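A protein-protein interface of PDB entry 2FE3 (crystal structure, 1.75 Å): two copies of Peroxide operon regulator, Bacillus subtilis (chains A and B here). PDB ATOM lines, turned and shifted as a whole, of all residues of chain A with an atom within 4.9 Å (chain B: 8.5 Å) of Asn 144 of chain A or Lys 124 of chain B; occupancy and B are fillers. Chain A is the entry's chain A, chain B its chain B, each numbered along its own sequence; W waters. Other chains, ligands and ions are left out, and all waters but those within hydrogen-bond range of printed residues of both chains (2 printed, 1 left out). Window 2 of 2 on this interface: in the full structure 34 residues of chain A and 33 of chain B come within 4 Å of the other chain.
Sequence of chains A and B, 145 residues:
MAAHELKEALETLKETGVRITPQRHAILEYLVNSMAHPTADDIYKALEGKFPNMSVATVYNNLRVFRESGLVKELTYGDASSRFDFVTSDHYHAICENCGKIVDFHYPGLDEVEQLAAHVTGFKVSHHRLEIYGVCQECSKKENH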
ATOM      1  N   TYR A 133     -19.799   8.372  13.593  1.00  0.00           N
ATOM      2  CA  TYR A 133     -20.741   8.755  12.549  1.00  0.00           C
ATOM      3  C   TYR A 133     -20.197   8.348  11.201  1.00  0.00           C
ATOM      4  O   TYR A 133     -18.988   8.407  10.961  1.00  0.00           O
ATOM      5  CB  TYR A 133     -21.008  10.258  12.558  1.00  0.00           C
ATOM      6  CG  TYR A 133     -21.668  10.694  13.827  1.00  0.00           C
ATOM      7  CD1 TYR A 133     -20.900  11.143  14.902  1.00  0.00           C
ATOM      8  CD2 TYR A 133     -23.056  10.644  13.961  1.00  0.00           C
ATOM      9  CE1 TYR A 133     -21.499  11.514  16.096  1.00  0.00           C
ATOM     10  CE2 TYR A 133     -23.663  11.032  15.136  1.00  0.00           C
ATOM     11  CZ  TYR A 133     -22.868  11.460  16.199  1.00  0.00           C
ATOM     12  OH  TYR A 133     -23.482  11.863  17.360  1.00  0.00           O
ATOM     13  N   GLY A 134     -21.097   7.868  10.343  1.00  0.00           N
ATOM     14  CA  GLY A 134     -20.685   7.488   9.008  1.00  0.00           C
ATOM     15  C   GLY A 134     -21.869   6.938   8.243  1.00  0.00           C
ATOM     16  O   GLY A 134     -22.993   7.406   8.411  1.00  0.00           O
ATOM     17  N   VAL A 135     -21.601   5.976   7.375  1.00  0.00           N
ATOM     18  CA  VAL A 135     -22.663   5.433   6.516  1.00  0.00           C
ATOM     19  C   VAL A 135     -22.694   3.926   6.685  1.00  0.00           C
ATOM     20  O   VAL A 135     -21.658   3.266   6.526  1.00  0.00           O
ATOM     21  CB  VAL A 135     -22.422   5.848   5.032  1.00  0.00           C
ATOM     22  CG1 VAL A 135     -23.471   5.185   4.141  1.00  0.00           C
ATOM     23  CG2 VAL A 135     -22.531   7.375   4.914  1.00  0.00           C
ATOM     24  N   SER A 140     -24.362   2.411   2.044  1.00  0.00           N
ATOM     25  CA  SER A 140     -23.155   2.418   1.236  1.00  0.00           C
ATOM     26  C   SER A 140     -23.371   1.600  -0.045  1.00  0.00           C
ATOM     27  O   SER A 140     -23.022   2.035  -1.128  1.00  0.00           O
ATOM     28  CB  SER A 140     -21.983   1.873   2.049  1.00  0.00           C
ATOM     29  OG  SER A 140     -20.786   1.944   1.307  1.00  0.00           O
ATOM     30  N   LYS A 141     -23.983   0.424   0.093  1.00  0.00           N
ATOM     31  CA  LYS A 141     -24.299  -0.429  -1.083  1.00  0.00           C
ATOM     32  C   LYS A 141     -25.253   0.308  -2.045  1.00  0.00           C
ATOM     33  O   LYS A 141     -25.034   0.345  -3.275  1.00  0.00           O
ATOM     34  CB  LYS A 141     -24.937  -1.750  -0.606  1.00  0.00           C
ATOM     35  CG  LYS A 141     -25.219  -2.779  -1.704  1.00  0.00           C
ATOM     36  CD  LYS A 141     -26.244  -3.816  -1.195  1.00  0.00           C
ATOM     37  CE  LYS A 141     -26.575  -4.874  -2.264  1.00  0.00           C
ATOM     38  NZ  LYS A 141     -27.193  -6.110  -1.654  1.00  0.00           N
ATOM     39  N   LYS A 142     -26.302   0.896  -1.474  1.00  0.00           N
ATOM     40  CA  LYS A 142     -27.307   1.651  -2.233  1.00  0.00           C
ATOM     41  C   LYS A 142     -26.698   2.812  -3.029  1.00  0.00           C
ATOM     42  O   LYS A 142     -27.093   3.067  -4.171  1.00  0.00           O
ATOM     43  CB  LYS A 142     -28.362   2.189  -1.274  1.00  0.00           C
ATOM     44  CG  LYS A 142     -29.635   2.668  -1.910  1.00  0.00           C
ATOM     45  CD  LYS A 142     -30.597   3.149  -0.825  1.00  0.00           C
ATOM     46  CE  LYS A 142     -31.974   3.451  -1.397  1.00  0.00           C
ATOM     47  NZ  LYS A 142     -32.334   4.880  -1.087  1.00  0.00           N
ATOM     48  N   GLU A 143     -25.741   3.510  -2.417  1.00  0.00           N
ATOM     49  CA  GLU A 143     -25.150   4.707  -3.000  1.00  0.00           C
ATOM     50  C   GLU A 143     -23.863   4.434  -3.789  1.00  0.00           C
ATOM     51  O   GLU A 143     -23.241   5.376  -4.287  1.00  0.00           O
ATOM     52  CB  GLU A 143     -24.853   5.725  -1.905  1.00  0.00           C
ATOM     53  CG  GLU A 143     -26.085   6.227  -1.183  1.00  0.00           C
ATOM     54  CD  GLU A 143     -25.716   7.211  -0.072  1.00  0.00           C
ATOM     55  OE1 GLU A 143     -24.498   7.404   0.199  1.00  0.00           O
ATOM     56  OE2 GLU A 143     -26.643   7.807   0.506  1.00  0.00           O
ATOM     57  N   ASN A 144     -23.490   3.161  -3.901  1.00  0.00           N
ATOM     58  CA  ASN A 144     -22.328   2.725  -4.683  1.00  0.00           C
ATOM     59  C   ASN A 144     -21.021   3.251  -4.116  1.00  0.00           C
ATOM     60  O   ASN A 144     -20.736   3.071  -2.925  1.00  0.00           O
ATOM     61  CB  ASN A 144     -22.458   3.170  -6.147  1.00  0.00           C
ATOM     62  CG  ASN A 144     -21.527   2.420  -7.056  1.00  0.00           C
ATOM     63  OD1 ASN A 144     -21.287   1.231  -6.846  1.00  0.00           O
ATOM     64  ND2 ASN A 144     -20.991   3.100  -8.077  1.00  0.00           N
ATOM     65  N   MET B  35     -21.591  11.681  -2.494  1.00  0.00           N
ATOM     66  CA  MET B  35     -21.820  10.433  -1.746  1.00  0.00           C
ATOM     67  C   MET B  35     -20.512   9.682  -1.602  1.00  0.00           C
ATOM     68  O   MET B  35     -20.084   9.398  -0.489  1.00  0.00           O
ATOM     69  CB  MET B  35     -22.899   9.567  -2.417  1.00  0.00           C
ATOM     70  CG  MET B  35     -24.226  10.300  -2.520  1.00  0.00           C
ATOM     71  SD  MET B  35     -25.617   9.304  -3.089  1.00  0.00           S
ATOM     72  CE  MET B  35     -25.239   9.113  -4.833  1.00  0.00           C
ATOM     73  N   ALA B  36     -19.850   9.382  -2.716  1.00  0.00           N
ATOM     74  CA  ALA B  36     -18.514   8.783  -2.645  1.00  0.00           C
ATOM     75  C   ALA B  36     -17.433   9.855  -2.784  1.00  0.00           C
ATOM     76  O   ALA B  36     -17.712  10.975  -3.191  1.00  0.00           O
ATOM     77  CB  ALA B  36     -18.349   7.705  -3.714  1.00  0.00           C
ATOM     78  N   HIS B  37     -16.205   9.500  -2.452  1.00  0.00           N
ATOM     79  CA  HIS B  37     -15.077  10.410  -2.530  1.00  0.00           C
ATOM     80  C   HIS B  37     -14.719  10.625  -3.980  1.00  0.00           C
ATOM     81  O   HIS B  37     -14.290   9.683  -4.652  1.00  0.00           O
ATOM     82  CB  HIS B  37     -13.905   9.805  -1.776  1.00  0.00           C
ATOM     83  CG  HIS B  37     -14.238   9.467  -0.359  1.00  0.00           C
ATOM     84  ND1 HIS B  37     -15.022  10.285   0.425  1.00  0.00           N
ATOM     85  CD2 HIS B  37     -13.892   8.415   0.418  1.00  0.00           C
ATOM     86  CE1 HIS B  37     -15.144   9.751   1.627  1.00  0.00           C
ATOM     87  NE2 HIS B  37     -14.463   8.620   1.651  1.00  0.00           N
ATOM     88  N   ASP B  85     -11.919  13.585   0.283  1.00  0.00           N
ATOM     89  CA  ASP B  85     -12.916  13.347   1.314  1.00  0.00           C
ATOM     90  C   ASP B  85     -13.082  14.676   2.057  1.00  0.00           C
ATOM     91  O   ASP B  85     -12.107  15.240   2.534  1.00  0.00           O
ATOM     92  CB  ASP B  85     -12.426  12.234   2.258  1.00  0.00           C
ATOM     93  CG  ASP B  85     -13.439  11.871   3.351  1.00  0.00           C
ATOM     94  OD1 ASP B  85     -14.572  12.402   3.351  1.00  0.00           O
ATOM     95  OD2 ASP B  85     -13.100  11.021   4.218  1.00  0.00           O
ATOM     96  N   GLU B 114     -11.771   3.510  15.286  1.00  0.00           N
ATOM     97  CA  GLU B 114     -12.500   3.709  14.016  1.00  0.00           C
ATOM     98  C   GLU B 114     -12.284   2.530  13.064  1.00  0.00           C
ATOM     99  O   GLU B 114     -13.225   2.053  12.428  1.00  0.00           O
ATOM    100  CB  GLU B 114     -12.072   5.014  13.344  1.00  0.00           C
ATOM    101  CG  GLU B 114     -12.619   6.266  14.049  1.00  0.00           C
ATOM    102  CD  GLU B 114     -12.501   7.518  13.183  1.00  0.00           C
ATOM    103  OE1 GLU B 114     -11.792   7.464  12.150  1.00  0.00           O
ATOM    104  OE2 GLU B 114     -13.130   8.556  13.519  1.00  0.00           O
ATOM    105  N   ALA B 117     -14.167  -0.473  14.497  1.00  0.00           N
ATOM    106  CA  ALA B 117     -15.612  -0.230  14.372  1.00  0.00           C
ATOM    107  C   ALA B 117     -16.103  -0.448  12.942  1.00  0.00           C
ATOM    108  O   ALA B 117     -17.143  -1.054  12.722  1.00  0.00           O
ATOM    109  CB  ALA B 117     -15.966   1.195  14.832  1.00  0.00           C
ATOM    110  N   ALA B 118     -15.344   0.038  11.969  1.00  0.00           N
ATOM    111  CA  ALA B 118     -15.750  -0.136  10.579  1.00  0.00           C
ATOM    112  C   ALA B 118     -15.793  -1.639  10.257  1.00  0.00           C
ATOM    113  O   ALA B 118     -16.689  -2.114   9.554  1.00  0.00           O
ATOM    114  CB  ALA B 118     -14.808   0.597   9.644  1.00  0.00           C
ATOM    115  N   HIS B 119     -14.839  -2.390  10.794  1.00  0.00           N
ATOM    116  CA  HIS B 119     -14.778  -3.822  10.496  1.00  0.00           C
ATOM    117  C   HIS B 119     -15.954  -4.583  11.108  1.00  0.00           C
ATOM    118  O   HIS B 119     -16.594  -5.421  10.430  1.00  0.00           O
ATOM    119  CB  HIS B 119     -13.458  -4.442  10.950  1.00  0.00           C
ATOM    120  CG  HIS B 119     -13.452  -5.935  10.813  1.00  0.00           C
ATOM    121  ND1 HIS B 119     -13.514  -6.781  11.893  1.00  0.00           N
ATOM    122  CD2 HIS B 119     -13.500  -6.722   9.715  1.00  0.00           C
ATOM    123  CE1 HIS B 119     -13.555  -8.033  11.474  1.00  0.00           C
ATOM    124  NE2 HIS B 119     -13.542  -8.025  10.154  1.00  0.00           N
ATOM    125  N   THR B 121     -18.864  -3.387  12.310  1.00  0.00           N
ATOM    126  CA  THR B 121     -20.222  -2.857  12.024  1.00  0.00           C
ATOM    127  C   THR B 121     -20.520  -2.792  10.508  1.00  0.00           C
ATOM    128  O   THR B 121     -21.697  -2.732  10.112  1.00  0.00           O
ATOM    129  CB  THR B 121     -20.425  -1.423  12.595  1.00  0.00           C
ATOM    130  OG1 THR B 121     -19.621  -0.511  11.847  1.00  0.00           O
ATOM    131  CG2 THR B 121     -20.098  -1.335  14.084  1.00  0.00           C
ATOM    132  N   GLY B 122     -19.470  -2.800   9.677  1.00  0.00           N
ATOM    133  CA  GLY B 122     -19.618  -2.568   8.240  1.00  0.00           C
ATOM    134  C   GLY B 122     -19.761  -1.114   7.791  1.00  0.00           C
ATOM    135  O   GLY B 122     -19.935  -0.847   6.599  1.00  0.00           O
ATOM    136  N   PHE B 123     -19.711  -0.166   8.731  1.00  0.00           N
ATOM    137  CA  PHE B 123     -19.835   1.256   8.409  1.00  0.00           C
ATOM    138  C   PHE B 123     -18.605   1.818   7.713  1.00  0.00           C
ATOM    139  O   PHE B 123     -17.480   1.371   7.986  1.00  0.00           O
ATOM    140  CB  PHE B 123     -20.011   2.063   9.693  1.00  0.00           C
ATOM    141  CG  PHE B 123     -21.421   2.161  10.173  1.00  0.00           C
ATOM    142  CD1 PHE B 123     -22.175   1.017  10.415  1.00  0.00           C
ATOM    143  CD2 PHE B 123     -21.980   3.411  10.459  1.00  0.00           C
ATOM    144  CE1 PHE B 123     -23.482   1.128  10.887  1.00  0.00           C
ATOM    145  CE2 PHE B 123     -23.296   3.512  10.936  1.00  0.00           C
ATOM    146  CZ  PHE B 123     -24.024   2.385  11.161  1.00  0.00           C
ATOM    147  N   LYS B 124     -18.827   2.781   6.824  1.00  0.00           N
ATOM    148  CA  LYS B 124     -17.771   3.702   6.362  1.00  0.00           C
ATOM    149  C   LYS B 124     -17.761   4.912   7.304  1.00  0.00           C
ATOM    150  O   LYS B 124     -18.777   5.602   7.441  1.00  0.00           O
ATOM    151  CB  LYS B 124     -17.997   4.140   4.894  1.00  0.00           C
ATOM    152  CG  LYS B 124     -17.596   3.057   3.843  1.00  0.00           C
ATOM    153  CD  LYS B 124     -17.867   3.548   2.392  1.00  0.00           C
ATOM    154  CE  LYS B 124     -17.709   2.431   1.348  1.00  0.00           C
ATOM    155  NZ  LYS B 124     -18.229   2.825  -0.017  1.00  0.00           N
ATOM    156  N   VAL B 125     -16.633   5.124   7.978  1.00  0.00           N
ATOM    157  CA  VAL B 125     -16.545   6.080   9.079  1.00  0.00           C
ATOM    158  C   VAL B 125     -16.212   7.486   8.590  1.00  0.00           C
ATOM    159  O   VAL B 125     -15.330   7.650   7.749  1.00  0.00           O
ATOM    160  CB  VAL B 125     -15.498   5.629  10.150  1.00  0.00           C
ATOM    161  CG1 VAL B 125     -15.265   6.749  11.211  1.00  0.00           C
ATOM    162  CG2 VAL B 125     -15.961   4.335  10.813  1.00  0.00           C
ATOM    163  N   SER B 126     -16.925   8.481   9.135  1.00  0.00           N
ATOM    164  CA  SER B 126     -16.667   9.904   8.870  1.00  0.00           C
ATOM    165  C   SER B 126     -15.954  10.594  10.034  1.00  0.00           C
ATOM    166  O   SER B 126     -14.892  11.174   9.860  1.00  0.00           O
ATOM    167  CB  SER B 126     -17.967  10.644   8.596  1.00  0.00           C
ATOM    168  OG  SER B 126     -17.733  12.044   8.489  1.00  0.00           O
ATOM    169  N   HIS B 127     -16.575  10.556  11.212  1.00  0.00           N
ATOM    170  CA  HIS B 127     -16.050  11.285  12.361  1.00  0.00           C
ATOM    171  C   HIS B 127     -16.661  10.754  13.651  1.00  0.00           C
ATOM    172  O   HIS B 127     -17.507   9.878  13.632  1.00  0.00           O
ATOM    173  CB  HIS B 127     -16.353  12.775  12.242  1.00  0.00           C
ATOM    174  CG  HIS B 127     -17.818  13.080  12.154  1.00  0.00           C
ATOM    175  ND1 HIS B 127     -18.559  12.837  11.018  1.00  0.00           N
ATOM    176  CD2 HIS B 127     -18.683  13.568  13.073  1.00  0.00           C
ATOM    177  CE1 HIS B 127     -19.813  13.197  11.229  1.00  0.00           C
ATOM    178  NE2 HIS B 127     -19.917  13.622  12.475  1.00  0.00           N
HETATM  179  O   HOH W   1     -21.497   7.291  -4.763  1.00  0.00           O
HETATM  180  O   HOH W   2     -20.539   0.922   4.698  1.00  0.00           O
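N of Ser 126 of chain B lies within hydrogen-bond range of O of Tyr 133 of chain A, at 2.8 Å. O of His 127 of chain B sits at hydrogen-bond distance from N of Tyr 133 of chain A (2.7 Å). OG of Ser 140 of chain A sits at hydrogen-bond distance from NZ of Lys 124 of chain B (3.0 Å). The backbone NH (N) of Val 135 of chain A is in hydrogen-bond range of the backbone carbonyl oxygen (O) of Lys 124 of chain B, 2.8 Å away.
N of Phe 123 of chain B sits at hydrogen-bond distance from OG1 of Thr 121 of chain B (3.1 Å). The side-chain hydroxyl (OG) of Ser 126 of chain B lies within hydrogen-bond range of a ring nitrogen (ND1) of His 127 of chain B (2.8 Å).
Among the printed residues, merely in contact across the chains: Gly 134 of chain A with Lys 124 of chain B (3.1 Å), Val 135 of chain A with Phe 123 of chain B (3.3 Å), Glu 143 of chain A with Met 35 of chain B (3.6 Å), Tyr 133 of chain A with Val 125 of chain B (3.8 Å), Asn 144 of chain A with Lys 124 of chain B (3.8 Å) and Gly 134 of chain A with Ser 126 of chain B (3.9 Å).
Of the printed residues of chain A, Lys 124 of chain B touches Gly 134 (3.1 Å), Val 135 (2.8 Å), Ser 140 (3.0 Å) and Asn 144 (3.8 Å). Of the printed residues of chain A, Phe 123 of chain B touches Val 135 (3.3 Å). Of the printed residues of chain A, Val 125 of chain B touches Tyr 133. Printed residues of chain B within 4 Å of Glu 143 of chain A: Met 35. Of the printed residues of chain B, Tyr 133 of chain A touches Val 125, Ser 126 and His 127. Asp 85 of chain B touches none of the printed residues of chain A. The nearest printed residue of chain A that does not touch Lys 124 of chain B is Tyr 133 of chain A (4.5 Å).
Of the 8 printed residues of chain A, 6 touch a printed residue of chain B. Of the 15 printed residues of chain B, 6 touch a printed residue of chain A. Printed residues of chain B that touch a printed residue of chain A: Met 35, Phe 123, Lys 124, Val 125, Ser 126 and His 127. Among the printed residues, no Asp or Glu carboxylate lies within 4 Å of a Lys or Arg side-chain nitrogen of the other chain.
No position is printed for both chains.
Water W1 lies within hydrogen-bond range of O of Glu 143 of chain A (2.6 Å) and N of Ala 36 of chain B (3.4 Å). Water W2 lies within hydrogen-bond range of the backbone carbonyl oxygen (O) of Gly 122 of chain B, the backbone carbonyl oxygen (O) of Val 135 of chain A and the backbone NH (N) of Lys 124 of chain B.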
